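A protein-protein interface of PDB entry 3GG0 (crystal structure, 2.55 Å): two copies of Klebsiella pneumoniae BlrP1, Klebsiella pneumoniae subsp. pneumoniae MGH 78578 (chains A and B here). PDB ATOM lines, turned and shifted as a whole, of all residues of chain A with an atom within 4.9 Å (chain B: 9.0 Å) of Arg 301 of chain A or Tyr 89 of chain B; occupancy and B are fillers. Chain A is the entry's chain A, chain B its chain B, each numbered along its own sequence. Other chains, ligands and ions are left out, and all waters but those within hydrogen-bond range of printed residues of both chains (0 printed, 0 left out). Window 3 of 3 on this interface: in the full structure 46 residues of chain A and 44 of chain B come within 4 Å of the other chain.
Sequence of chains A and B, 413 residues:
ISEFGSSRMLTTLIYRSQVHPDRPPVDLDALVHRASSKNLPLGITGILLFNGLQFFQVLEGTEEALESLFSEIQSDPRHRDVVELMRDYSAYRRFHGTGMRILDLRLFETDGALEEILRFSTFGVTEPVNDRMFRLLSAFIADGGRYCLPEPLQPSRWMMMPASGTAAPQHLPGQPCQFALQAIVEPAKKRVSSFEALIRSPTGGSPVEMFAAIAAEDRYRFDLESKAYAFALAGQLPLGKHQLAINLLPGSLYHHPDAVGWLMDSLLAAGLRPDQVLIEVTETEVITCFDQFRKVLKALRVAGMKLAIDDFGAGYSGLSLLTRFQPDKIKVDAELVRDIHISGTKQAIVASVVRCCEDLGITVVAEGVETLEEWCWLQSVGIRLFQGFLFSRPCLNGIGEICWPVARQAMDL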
ATOM      1  N   LEU A 297      -2.008  15.714  30.550  1.00  0.00           N
ATOM      2  CA  LEU A 297      -1.377  14.457  30.141  1.00  0.00           C
ATOM      3  C   LEU A 297       0.104  14.652  29.830  1.00  0.00           C
ATOM      4  O   LEU A 297       0.950  13.896  30.309  1.00  0.00           O
ATOM      5  CB  LEU A 297      -2.100  13.859  28.926  1.00  0.00           C
ATOM      6  CG  LEU A 297      -1.417  12.674  28.220  1.00  0.00           C
ATOM      7  CD1 LEU A 297      -2.410  11.553  27.957  1.00  0.00           C
ATOM      8  CD2 LEU A 297      -0.712  13.105  26.915  1.00  0.00           C
ATOM      9  N   LYS A 298       0.408  15.675  29.031  1.00  0.00           N
ATOM     10  CA  LYS A 298       1.788  16.003  28.680  1.00  0.00           C
ATOM     11  C   LYS A 298       2.631  16.319  29.917  1.00  0.00           C
ATOM     12  O   LYS A 298       3.779  15.897  30.015  1.00  0.00           O
ATOM     13  CB  LYS A 298       1.829  17.175  27.693  1.00  0.00           C
ATOM     14  CG  LYS A 298       3.207  17.455  27.108  1.00  0.00           C
ATOM     15  CD  LYS A 298       3.133  18.492  25.995  1.00  0.00           C
ATOM     16  CE  LYS A 298       4.515  19.008  25.620  1.00  0.00           C
ATOM     17  NZ  LYS A 298       5.159  19.744  26.748  1.00  0.00           N
ATOM     18  N   ALA A 299       2.046  17.045  30.867  1.00  0.00           N
ATOM     19  CA  ALA A 299       2.738  17.375  32.112  1.00  0.00           C
ATOM     20  C   ALA A 299       2.990  16.136  32.978  1.00  0.00           C
ATOM     21  O   ALA A 299       4.039  16.017  33.601  1.00  0.00           O
ATOM     22  CB  ALA A 299       1.967  18.427  32.888  1.00  0.00           C
ATOM     23  N   LEU A 300       2.030  15.213  32.991  1.00  0.00           N
ATOM     24  CA  LEU A 300       2.161  13.964  33.753  1.00  0.00           C
ATOM     25  C   LEU A 300       3.224  13.036  33.161  1.00  0.00           C
ATOM     26  O   LEU A 300       3.966  12.382  33.895  1.00  0.00           O
ATOM     27  CB  LEU A 300       0.818  13.229  33.825  1.00  0.00           C
ATOM     28  CG  LEU A 300      -0.303  13.851  34.661  1.00  0.00           C
ATOM     29  CD1 LEU A 300      -1.613  13.137  34.397  1.00  0.00           C
ATOM     30  CD2 LEU A 300       0.034  13.816  36.134  1.00  0.00           C
ATOM     31  N   ARG A 301       3.285  12.979  31.832  1.00  0.00           N
ATOM     32  CA  ARG A 301       4.273  12.152  31.138  1.00  0.00           C
ATOM     33  C   ARG A 301       5.687  12.688  31.334  1.00  0.00           C
ATOM     34  O   ARG A 301       6.623  11.917  31.566  1.00  0.00           O
ATOM     35  CB  ARG A 301       3.952  12.066  29.644  1.00  0.00           C
ATOM     36  CG  ARG A 301       2.769  11.177  29.309  1.00  0.00           C
ATOM     37  CD  ARG A 301       3.159   9.706  29.290  1.00  0.00           C
ATOM     38  NE  ARG A 301       2.035   8.858  28.906  1.00  0.00           N
ATOM     39  CZ  ARG A 301       1.164   8.335  29.766  1.00  0.00           C
ATOM     40  NH1 ARG A 301       1.288   8.565  31.067  1.00  0.00           N
ATOM     41  NH2 ARG A 301       0.172   7.578  29.326  1.00  0.00           N
ATOM     42  N   VAL A 302       5.834  14.011  31.235  1.00  0.00           N
ATOM     43  CA  VAL A 302       7.132  14.674  31.410  1.00  0.00           C
ATOM     44  C   VAL A 302       7.636  14.558  32.855  1.00  0.00           C
ATOM     45  O   VAL A 302       8.827  14.329  33.089  1.00  0.00           O
ATOM     46  CB  VAL A 302       7.076  16.171  30.972  1.00  0.00           C
ATOM     47  CG1 VAL A 302       8.260  16.951  31.530  1.00  0.00           C
ATOM     48  CG2 VAL A 302       7.035  16.280  29.457  1.00  0.00           C
ATOM     49  N   ALA A 303       6.721  14.685  33.816  1.00  0.00           N
ATOM     50  CA  ALA A 303       7.068  14.537  35.228  1.00  0.00           C
ATOM     51  C   ALA A 303       7.441  13.095  35.569  1.00  0.00           C
ATOM     52  O   ALA A 303       8.304  12.853  36.409  1.00  0.00           O
ATOM     53  CB  ALA A 303       5.939  15.009  36.101  1.00  0.00           C
ATOM     54  N   GLY A 304       6.790  12.141  34.908  1.00  0.00           N
ATOM     55  CA  GLY A 304       7.088  10.729  35.115  1.00  0.00           C
ATOM     56  C   GLY A 304       5.960   9.957  35.774  1.00  0.00           C
ATOM     57  O   GLY A 304       6.062   8.748  35.975  1.00  0.00           O
ATOM     58  N   MET A 305       4.882  10.658  36.113  1.00  0.00           N
ATOM     59  CA  MET A 305       3.706  10.015  36.691  1.00  0.00           C
ATOM     60  C   MET A 305       2.929   9.223  35.639  1.00  0.00           C
ATOM     61  O   MET A 305       2.820   9.643  34.488  1.00  0.00           O
ATOM     62  CB  MET A 305       2.801  11.048  37.361  1.00  0.00           C
ATOM     63  CG  MET A 305       3.326  11.545  38.692  1.00  0.00           C
ATOM     64  SD  MET A 305       2.338  12.883  39.374  1.00  0.00           S
ATOM     65  CE  MET A 305       2.993  14.281  38.487  1.00  0.00           C
ATOM     66  N   LYS A 306       2.399   8.074  36.043  1.00  0.00           N
ATOM     67  CA  LYS A 306       1.652   7.218  35.131  1.00  0.00           C
ATOM     68  C   LYS A 306       0.156   7.512  35.179  1.00  0.00           C
ATOM     69  O   LYS A 306      -0.355   8.033  36.168  1.00  0.00           O
ATOM     70  CB  LYS A 306       1.921   5.741  35.434  1.00  0.00           C
ATOM     71  CG  LYS A 306       3.336   5.289  35.101  1.00  0.00           C
ATOM     72  CD  LYS A 306       3.434   3.776  35.064  1.00  0.00           C
ATOM     73  CE  LYS A 306       4.859   3.306  35.335  1.00  0.00           C
ATOM     74  NZ  LYS A 306       5.755   3.500  34.163  1.00  0.00           N
ATOM     75  N   LEU A 307      -0.540   7.184  34.095  1.00  0.00           N
ATOM     76  CA  LEU A 307      -1.970   7.436  33.995  1.00  0.00           C
ATOM     77  C   LEU A 307      -2.744   6.138  33.837  1.00  0.00           C
ATOM     78  O   LEU A 307      -2.324   5.237  33.112  1.00  0.00           O
ATOM     79  CB  LEU A 307      -2.267   8.368  32.820  1.00  0.00           C
ATOM     80  CG  LEU A 307      -3.736   8.733  32.589  1.00  0.00           C
ATOM     81  CD1 LEU A 307      -4.212   9.742  33.626  1.00  0.00           C
ATOM     82  CD2 LEU A 307      -3.945   9.265  31.179  1.00  0.00           C
ATOM     83  N   GLN A 326      -2.891   7.003  24.918  1.00  0.00           N
ATOM     84  CA  GLN A 326      -2.801   5.699  25.569  1.00  0.00           C
ATOM     85  C   GLN A 326      -2.393   5.844  27.017  1.00  0.00           C
ATOM     86  O   GLN A 326      -1.354   6.419  27.313  1.00  0.00           O
ATOM     87  CB  GLN A 326      -1.816   4.782  24.839  1.00  0.00           C
ATOM     88  CG  GLN A 326      -2.155   4.528  23.384  1.00  0.00           C
ATOM     89  CD  GLN A 326      -1.615   5.606  22.471  1.00  0.00           C
ATOM     90  OE1 GLN A 326      -0.413   5.875  22.452  1.00  0.00           O
ATOM     91  NE2 GLN A 326      -2.501   6.237  21.710  1.00  0.00           N
ATOM     92  N   PRO A 327      -3.215   5.310  27.933  1.00  0.00           N
ATOM     93  CA  PRO A 327      -2.862   5.261  29.343  1.00  0.00           C
ATOM     94  C   PRO A 327      -1.800   4.203  29.606  1.00  0.00           C
ATOM     95  O   PRO A 327      -1.477   3.409  28.720  1.00  0.00           O
ATOM     96  CB  PRO A 327      -4.176   4.856  30.011  1.00  0.00           C
ATOM     97  CG  PRO A 327      -4.877   4.064  28.987  1.00  0.00           C
ATOM     98  CD  PRO A 327      -4.535   4.708  27.675  1.00  0.00           C
ATOM     99  N   ASP A 328      -1.254   4.202  30.812  1.00  0.00           N
ATOM    100  CA  ASP A 328      -0.370   3.139  31.232  1.00  0.00           C
ATOM    101  C   ASP A 328      -1.191   1.943  31.692  1.00  0.00           C
ATOM    102  O   ASP A 328      -0.822   0.797  31.448  1.00  0.00           O
ATOM    103  CB  ASP A 328       0.558   3.622  32.348  1.00  0.00           C
ATOM    104  CG  ASP A 328       1.656   4.533  31.836  1.00  0.00           C
ATOM    105  OD1 ASP A 328       2.634   4.017  31.260  1.00  0.00           O
ATOM    106  OD2 ASP A 328       1.546   5.767  32.011  1.00  0.00           O
ATOM    107  N   MET B   9      13.029  18.474  24.711  1.00  0.00           N
ATOM    108  CA  MET B   9      12.551  17.544  25.779  1.00  0.00           C
ATOM    109  C   MET B   9      12.517  16.098  25.290  1.00  0.00           C
ATOM    110  O   MET B   9      12.412  15.839  24.091  1.00  0.00           O
ATOM    111  CB  MET B   9      11.169  17.969  26.291  1.00  0.00           C
ATOM    112  CG  MET B   9      10.142  18.237  25.192  1.00  0.00           C
ATOM    113  SD  MET B   9       8.521  18.729  25.841  1.00  0.00           S
ATOM    114  CE  MET B   9       8.978  20.091  26.925  1.00  0.00           C
ATOM    115  N   LEU B  10      12.592  15.162  26.232  1.00  0.00           N
ATOM    116  CA  LEU B  10      12.799  13.751  25.913  1.00  0.00           C
ATOM    117  C   LEU B  10      11.559  13.093  25.302  1.00  0.00           C
ATOM    118  O   LEU B  10      10.436  13.346  25.728  1.00  0.00           O
ATOM    119  CB  LEU B  10      13.244  12.988  27.160  1.00  0.00           C
ATOM    120  CG  LEU B  10      13.938  11.638  26.958  1.00  0.00           C
ATOM    121  CD1 LEU B  10      15.122  11.759  26.013  1.00  0.00           C
ATOM    122  CD2 LEU B  10      14.379  11.078  28.291  1.00  0.00           C
ATOM    123  N   THR B  11      11.787  12.247  24.303  1.00  0.00           N
ATOM    124  CA  THR B  11      10.713  11.569  23.589  1.00  0.00           C
ATOM    125  C   THR B  11      11.054  10.089  23.428  1.00  0.00           C
ATOM    126  O   THR B  11      12.227   9.716  23.383  1.00  0.00           O
ATOM    127  CB  THR B  11      10.486  12.204  22.186  1.00  0.00           C
ATOM    128  OG1 THR B  11      10.216  13.604  22.328  1.00  0.00           O
ATOM    129  CG2 THR B  11       9.315  11.546  21.464  1.00  0.00           C
ATOM    130  N   THR B  12      10.025   9.251  23.383  1.00  0.00           N
ATOM    131  CA  THR B  12      10.180   7.855  23.007  1.00  0.00           C
ATOM    132  C   THR B  12       9.570   7.643  21.633  1.00  0.00           C
ATOM    133  O   THR B  12       8.521   8.198  21.321  1.00  0.00           O
ATOM    134  CB  THR B  12       9.464   6.919  24.002  1.00  0.00           C
ATOM    135  OG1 THR B  12       9.785   7.298  25.347  1.00  0.00           O
ATOM    136  CG2 THR B  12       9.876   5.472  23.771  1.00  0.00           C
ATOM    137  N   LEU B  13      10.227   6.843  20.809  1.00  0.00           N
ATOM    138  CA  LEU B  13       9.650   6.438  19.549  1.00  0.00           C
ATOM    139  C   LEU B  13       9.912   4.967  19.312  1.00  0.00           C
ATOM    140  O   LEU B  13      11.056   4.547  19.157  1.00  0.00           O
ATOM    141  CB  LEU B  13      10.206   7.285  18.403  1.00  0.00           C
ATOM    142  CG  LEU B  13       9.771   6.934  16.975  1.00  0.00           C
ATOM    143  CD1 LEU B  13       8.319   7.310  16.728  1.00  0.00           C
ATOM    144  CD2 LEU B  13      10.675   7.629  15.979  1.00  0.00           C
ATOM    145  N   GLU B  60      15.231   6.803  21.886  1.00  0.00           N
ATOM    146  CA  GLU B  60      15.058   7.862  22.879  1.00  0.00           C
ATOM    147  C   GLU B  60      15.880   9.091  22.515  1.00  0.00           C
ATOM    148  O   GLU B  60      17.045   8.984  22.155  1.00  0.00           O
ATOM    149  CB  GLU B  60      15.443   7.368  24.276  1.00  0.00           C
ATOM    150  CG  GLU B  60      14.709   6.119  24.722  1.00  0.00           C
ATOM    151  CD  GLU B  60      15.065   5.702  26.139  1.00  0.00           C
ATOM    152  OE1 GLU B  60      16.267   5.500  26.426  1.00  0.00           O
ATOM    153  OE2 GLU B  60      14.138   5.566  26.965  1.00  0.00           O
ATOM    154  N   GLY B  61      15.262  10.259  22.613  1.00  0.00           N
ATOM    155  CA  GLY B  61      15.937  11.514  22.299  1.00  0.00           C
ATOM    156  C   GLY B  61      14.964  12.671  22.261  1.00  0.00           C
ATOM    157  O   GLY B  61      13.835  12.558  22.735  1.00  0.00           O
ATOM    158  N   THR B  62      15.401  13.791  21.698  1.00  0.00           N
ATOM    159  CA  THR B  62      14.535  14.957  21.560  1.00  0.00           C
ATOM    160  C   THR B  62      13.509  14.747  20.443  1.00  0.00           C
ATOM    161  O   THR B  62      13.712  13.917  19.546  1.00  0.00           O
ATOM    162  CB  THR B  62      15.343  16.236  21.299  1.00  0.00           C
ATOM    163  OG1 THR B  62      16.010  16.135  20.038  1.00  0.00           O
ATOM    164  CG2 THR B  62      16.375  16.448  22.401  1.00  0.00           C
ATOM    165  N   GLU B  63      12.404  15.487  20.512  1.00  0.00           N
ATOM    166  CA  GLU B  63      11.313  15.330  19.554  1.00  0.00           C
ATOM    167  C   GLU B  63      11.785  15.609  18.132  1.00  0.00           C
ATOM    168  O   GLU B  63      11.444  14.880  17.204  1.00  0.00           O
ATOM    169  CB  GLU B  63      10.147  16.252  19.912  1.00  0.00           C
ATOM    170  CG  GLU B  63       8.843  15.900  19.214  1.00  0.00           C
ATOM    171  CD  GLU B  63       7.791  16.986  19.350  1.00  0.00           C
ATOM    172  OE1 GLU B  63       8.105  18.158  19.047  1.00  0.00           O
ATOM    173  OE2 GLU B  63       6.645  16.663  19.748  1.00  0.00           O
ATOM    174  N   GLU B  64      12.593  16.653  17.979  1.00  0.00           N
ATOM    175  CA  GLU B  64      13.105  17.053  16.672  1.00  0.00           C
ATOM    176  C   GLU B  64      14.144  16.069  16.130  1.00  0.00           C
ATOM    177  O   GLU B  64      14.229  15.859  14.920  1.00  0.00           O
ATOM    178  CB  GLU B  64      13.693  18.464  16.736  1.00  0.00           C
ATOM    179  CG  GLU B  64      12.728  19.515  17.295  1.00  0.00           C
ATOM    180  CD  GLU B  64      13.421  20.828  17.657  1.00  0.00           C
ATOM    181  OE1 GLU B  64      14.637  20.974  17.361  1.00  0.00           O
ATOM    182  OE2 GLU B  64      12.747  21.716  18.236  1.00  0.00           O
ATOM    183  N   LEU B  66      14.279  12.700  16.893  1.00  0.00           N
ATOM    184  CA  LEU B  66      13.570  11.466  16.551  1.00  0.00           C
ATOM    185  C   LEU B  66      12.697  11.598  15.300  1.00  0.00           C
ATOM    186  O   LEU B  66      12.524  10.634  14.557  1.00  0.00           O
ATOM    187  CB  LEU B  66      12.739  10.971  17.738  1.00  0.00           C
ATOM    188  CG  LEU B  66      13.532  10.513  18.964  1.00  0.00           C
ATOM    189  CD1 LEU B  66      12.621   9.813  19.960  1.00  0.00           C
ATOM    190  CD2 LEU B  66      14.676   9.606  18.557  1.00  0.00           C
ATOM    191  N   GLU B  67      12.155  12.794  15.072  1.00  0.00           N
ATOM    192  CA  GLU B  67      11.388  13.076  13.850  1.00  0.00           C
ATOM    193  C   GLU B  67      12.274  12.996  12.606  1.00  0.00           C
ATOM    194  O   GLU B  67      11.897  12.390  11.599  1.00  0.00           O
ATOM    195  CB  GLU B  67      10.747  14.465  13.925  1.00  0.00           C
ATOM    196  CG  GLU B  67       9.415  14.518  14.651  1.00  0.00           C
ATOM    197  CD  GLU B  67       8.878  15.938  14.760  1.00  0.00           C
ATOM    198  OE1 GLU B  67       9.608  16.813  15.282  1.00  0.00           O
ATOM    199  OE2 GLU B  67       7.731  16.180  14.319  1.00  0.00           O
ATOM    200  N   MET B  86       4.523   3.310  19.450  1.00  0.00           N
ATOM    201  CA  MET B  86       4.512   4.236  20.572  1.00  0.00           C
ATOM    202  C   MET B  86       5.283   5.504  20.244  1.00  0.00           C
ATOM    203  O   MET B  86       6.379   5.450  19.689  1.00  0.00           O
ATOM    204  CB  MET B  86       5.102   3.568  21.817  1.00  0.00           C
ATOM    205  CG  MET B  86       5.144   4.457  23.035  1.00  0.00           C
ATOM    206  SD  MET B  86       5.895   3.646  24.452  1.00  0.00           S
ATOM    207  CE  MET B  86       5.834   4.972  25.669  1.00  0.00           C
ATOM    208  N   ARG B  87       4.694   6.643  20.579  1.00  0.00           N
ATOM    209  CA  ARG B  87       5.383   7.921  20.492  1.00  0.00           C
ATOM    210  C   ARG B  87       4.848   8.855  21.552  1.00  0.00           C
ATOM    211  O   ARG B  87       3.711   9.315  21.463  1.00  0.00           O
ATOM    212  CB  ARG B  87       5.208   8.546  19.105  1.00  0.00           C
ATOM    213  CG  ARG B  87       5.952   9.865  18.921  1.00  0.00           C
ATOM    214  CD  ARG B  87       5.329  10.707  17.820  1.00  0.00           C
ATOM    215  NE  ARG B  87       5.452  10.076  16.507  1.00  0.00           N
ATOM    216  CZ  ARG B  87       6.457  10.286  15.661  1.00  0.00           C
ATOM    217  NH1 ARG B  87       7.442  11.114  15.987  1.00  0.00           N
ATOM    218  NH2 ARG B  87       6.476   9.665  14.485  1.00  0.00           N
ATOM    219  N   ASP B  88       5.664   9.126  22.562  1.00  0.00           N
ATOM    220  CA  ASP B  88       5.245   9.969  23.669  1.00  0.00           C
ATOM    221  C   ASP B  88       6.441  10.645  24.338  1.00  0.00           C
ATOM    222  O   ASP B  88       7.593  10.275  24.098  1.00  0.00           O
ATOM    223  CB  ASP B  88       4.459   9.145  24.694  1.00  0.00           C
ATOM    224  CG  ASP B  88       3.186   9.842  25.153  1.00  0.00           C
ATOM    225  OD1 ASP B  88       3.114  11.089  25.069  1.00  0.00           O
ATOM    226  OD2 ASP B  88       2.254   9.139  25.598  1.00  0.00           O
ATOM    227  N   TYR B  89       6.160  11.644  25.169  1.00  0.00           N
ATOM    228  CA  TYR B  89       7.194  12.300  25.953  1.00  0.00           C
ATOM    229  C   TYR B  89       7.654  11.402  27.098  1.00  0.00           C
ATOM    230  O   TYR B  89       6.840  10.737  27.744  1.00  0.00           O
ATOM    231  CB  TYR B  89       6.688  13.641  26.493  1.00  0.00           C
ATOM    232  CG  TYR B  89       6.270  14.607  25.408  1.00  0.00           C
ATOM    233  CD1 TYR B  89       7.220  15.338  24.698  1.00  0.00           C
ATOM    234  CD2 TYR B  89       4.926  14.778  25.078  1.00  0.00           C
ATOM    235  CE1 TYR B  89       6.845  16.221  23.689  1.00  0.00           C
ATOM    236  CE2 TYR B  89       4.539  15.659  24.073  1.00  0.00           C
ATOM    237  CZ  TYR B  89       5.507  16.378  23.382  1.00  0.00           C
ATOM    238  OH  TYR B  89       5.139  17.251  22.385  1.00  0.00           O
ATOM    239  N   SER B  90       8.960  11.374  27.332  1.00  0.00           N
ATOM    240  CA  SER B  90       9.534  10.540  28.375  1.00  0.00           C
ATOM    241  C   SER B  90      10.164  11.393  29.475  1.00  0.00           C
ATOM    242  O   SER B  90      10.579  12.524  29.234  1.00  0.00           O
ATOM    243  CB  SER B  90      10.570   9.586  27.781  1.00  0.00           C
ATOM    244  OG  SER B  90      11.176   8.797  28.790  1.00  0.00           O
ATOM    245  N   ALA B  91      10.233  10.836  30.683  1.00  0.00           N
ATOM    246  CA  ALA B  91      10.778  11.548  31.839  1.00  0.00           C
ATOM    247  C   ALA B  91      12.252  11.210  32.069  1.00  0.00           C
ATOM    248  O   ALA B  91      13.004  12.008  32.629  1.00  0.00           O
ATOM    249  CB  ALA B  91       9.971  11.233  33.071  1.00  0.00           C
ATOM    250  N   TYR B  92      12.647  10.011  31.648  1.00  0.00           N
ATOM    251  CA  TYR B  92      14.014   9.532  31.825  1.00  0.00           C
ATOM    252  C   TYR B  92      14.358   8.548  30.719  1.00  0.00           C
ATOM    253  O   TYR B  92      13.478   7.870  30.189  1.00  0.00           O
ATOM    254  CB  TYR B  92      14.185   8.867  33.204  1.00  0.00           C
ATOM    255  CG  TYR B  92      13.394   7.583  33.383  1.00  0.00           C
ATOM    256  CD1 TYR B  92      12.052   7.614  33.769  1.00  0.00           C
ATOM    257  CD2 TYR B  92      13.993   6.339  33.178  1.00  0.00           C
ATOM    258  CE1 TYR B  92      11.321   6.440  33.932  1.00  0.00           C
ATOM    259  CE2 TYR B  92      13.274   5.158  33.341  1.00  0.00           C
ATOM    260  CZ  TYR B  92      11.938   5.215  33.717  1.00  0.00           C
ATOM    261  OH  TYR B  92      11.222   4.047  33.880  1.00  0.00           O
ATOM    262  N   ARG B  94      15.416   5.186  29.421  1.00  0.00           N
ATOM    263  CA  ARG B  94      15.479   3.789  29.828  1.00  0.00           C
ATOM    264  C   ARG B  94      16.797   3.176  29.379  1.00  0.00           C
ATOM    265  O   ARG B  94      17.398   2.386  30.097  1.00  0.00           O
ATOM    266  CB  ARG B  94      14.303   3.002  29.245  1.00  0.00           C
ATOM    267  CG  ARG B  94      13.008   3.110  30.042  1.00  0.00           C
ATOM    268  CD  ARG B  94      12.358   4.479  29.898  1.00  0.00           C
ATOM    269  NE  ARG B  94      10.975   4.480  30.367  1.00  0.00           N
ATOM    270  CZ  ARG B  94      10.287   5.578  30.671  1.00  0.00           C
ATOM    271  NH1 ARG B  94      10.857   6.775  30.572  1.00  0.00           N
ATOM    272  NH2 ARG B  94       9.032   5.482  31.090  1.00  0.00           N
ATOM    273  N   ARG B 132       5.550   0.720  29.920  1.00  0.00           N
ATOM    274  CA  ARG B 132       4.947   0.434  28.612  1.00  0.00           C
ATOM    275  C   ARG B 132       5.975  -0.018  27.577  1.00  0.00           C
ATOM    276  O   ARG B 132       5.709  -0.917  26.781  1.00  0.00           O
ATOM    277  CB  ARG B 132       4.174   1.662  28.104  1.00  0.00           C
ATOM    278  CG  ARG B 132       3.394   1.426  26.821  1.00  0.00           C
ATOM    279  CD  ARG B 132       2.227   2.396  26.674  1.00  0.00           C
ATOM    280  NE  ARG B 132       1.387   2.042  25.530  1.00  0.00           N
ATOM    281  CZ  ARG B 132       1.348   2.719  24.387  1.00  0.00           C
ATOM    282  NH1 ARG B 132       2.079   3.813  24.234  1.00  0.00           N
ATOM    283  NH2 ARG B 132       0.566   2.309  23.399  1.00  0.00           N
ATOM    284  N   MET B 133       7.147   0.606  27.601  1.00  0.00           N
ATOM    285  CA  MET B 133       8.247   0.233  26.718  1.00  0.00           C
ATOM    286  C   MET B 133       8.670  -1.230  26.933  1.00  0.00           C
ATOM    287  O   MET B 133       8.842  -1.986  25.973  1.00  0.00           O
ATOM    288  CB  MET B 133       9.437   1.166  26.943  1.00  0.00           C
ATOM    289  CG  MET B 133      10.599   0.940  25.999  1.00  0.00           C
ATOM    290  SD  MET B 133      12.079   1.833  26.507  1.00  0.00           S
ATOM    291  CE  MET B 133      11.496   3.527  26.442  1.00  0.00           C
ATOM    292  N   ARG B 135       6.894  -3.602  28.274  1.00  0.00           N
ATOM    293  CA  ARG B 135       5.779  -4.460  27.887  1.00  0.00           C
ATOM    294  C   ARG B 135       5.728  -4.679  26.372  1.00  0.00           C
ATOM    295  O   ARG B 135       5.478  -5.789  25.905  1.00  0.00           O
ATOM    296  CB  ARG B 135       4.455  -3.888  28.396  1.00  0.00           C
ATOM    297  CG  ARG B 135       4.311  -3.935  29.913  1.00  0.00           C
ATOM    298  CD  ARG B 135       2.906  -3.579  30.355  1.00  0.00           C
ATOM    299  NE  ARG B 135       2.569  -2.182  30.068  1.00  0.00           N
ATOM    300  CZ  ARG B 135       2.634  -1.187  30.956  1.00  0.00           C
ATOM    301  NH1 ARG B 135       3.032  -1.424  32.195  1.00  0.00           N
ATOM    302  NH2 ARG B 135       2.293   0.047  30.600  1.00  0.00           N
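The side-chain carboxylate (OD2) of Asp 88 of chain B is in salt-bridge range of the guanidinium group (NE) of Arg 301 of chain A.
The backbone carbonyl oxygen of Asp 328 of chain A sits at hydrogen-bond distance from the guanidinium group of Arg 135 of chain B (3.3 Å).
NZ of Lys 298 of chain A is in hydrogen-bond range of SD of Met 9 of chain B, at 3.6 Å.
The backbone carbonyl oxygen of Asp 88 of chain B lies within hydrogen-bond range of the backbone NH of Thr 12 of chain B, at 2.7 Å.
The side-chain hydroxyl (OH) of Tyr 89 of chain B is in hydrogen-bond range of the side-chain carboxylate (OE2) of Glu 63 of chain B.
The guanidinium group of Arg 301 of chain A lies within hydrogen-bond range of the backbone carbonyl oxygen of Gln 326 of chain A, at 2.8 Å.
The backbone NH (N) of Asp 328 of chain A sits at hydrogen-bond distance from the backbone carbonyl oxygen (O) of Leu 307 of chain A, 2.7 Å away.
Tyr 89 of chain B touches Lys 298 of chain A (CZ to CE, 3.6 Å).
O of Tyr 89 of chain B touches CB of Arg 301 of chain A (3.7 Å).
Ala 91 of chain B touches Arg 301 of chain A (CB to O, 3.7 Å).
Val 302 of chain A touches Tyr 89 of chain B (CG2 to CB, 3.98 Å).
Ala 91 of chain B touches Val 302 of chain A (CB to O, 3.3 Å).
Gly 304 of chain A touches Ala 91 of chain B.
Gln 326 of chain A touches Arg 132 of chain B.
Of chain B, only Met 9 (3.6 Å) and Tyr 89 (3.6 Å) come within 4 Å of Lys 298 of chain A.
Of the printed residues of chain B, Gly 304 of chain A touches Ala 91.
Printed residues of chain B within 4 Å of Asp 328 of chain A: Arg 135.
Printed residues of chain A within 4 Å of Asp 88 of chain B: Arg 301 (3.3 Å).
Printed residues of chain A within 4 Å of Tyr 89 of chain B: Lys 298, Arg 301 and Val 302.
Of the printed residues of chain A, Ala 91 of chain B touches Arg 301 (3.7 Å), Val 302 (3.3 Å) and Gly 304 (3.6 Å).
Printed residues of chain A within 4 Å of Arg 135 of chain B: Asp 328.
The nearest residue of chain B that does not touch Arg 301 of chain A is Ser 90 of chain B (4.1 Å).
The nearest printed residue of chain B that does not touch Asp 328 of chain A is Arg 132 of chain B (4.2 Å).
Of the 14 printed residues of chain A, 6 touch a printed residue of chain B.
Printed residues of chain A that touch a printed residue of chain B: Lys 298, Arg 301, Val 302, Gly 304, Gln 326 and Asp 328.
Hydrophobic or aromatic side chains of chain A within 4 Å of the printed part of chain B: Val 302.
Along chain A the printed residues that touch a printed residue of chain B span positions 298 to 328.
Among the printed residues, Asp or Glu carboxylates within 4 Å of a Lys or Arg side-chain nitrogen of the other chain: Arg 301 of chain A with Asp 88 of chain B (3.3 Å).
No position is printed for both chains.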
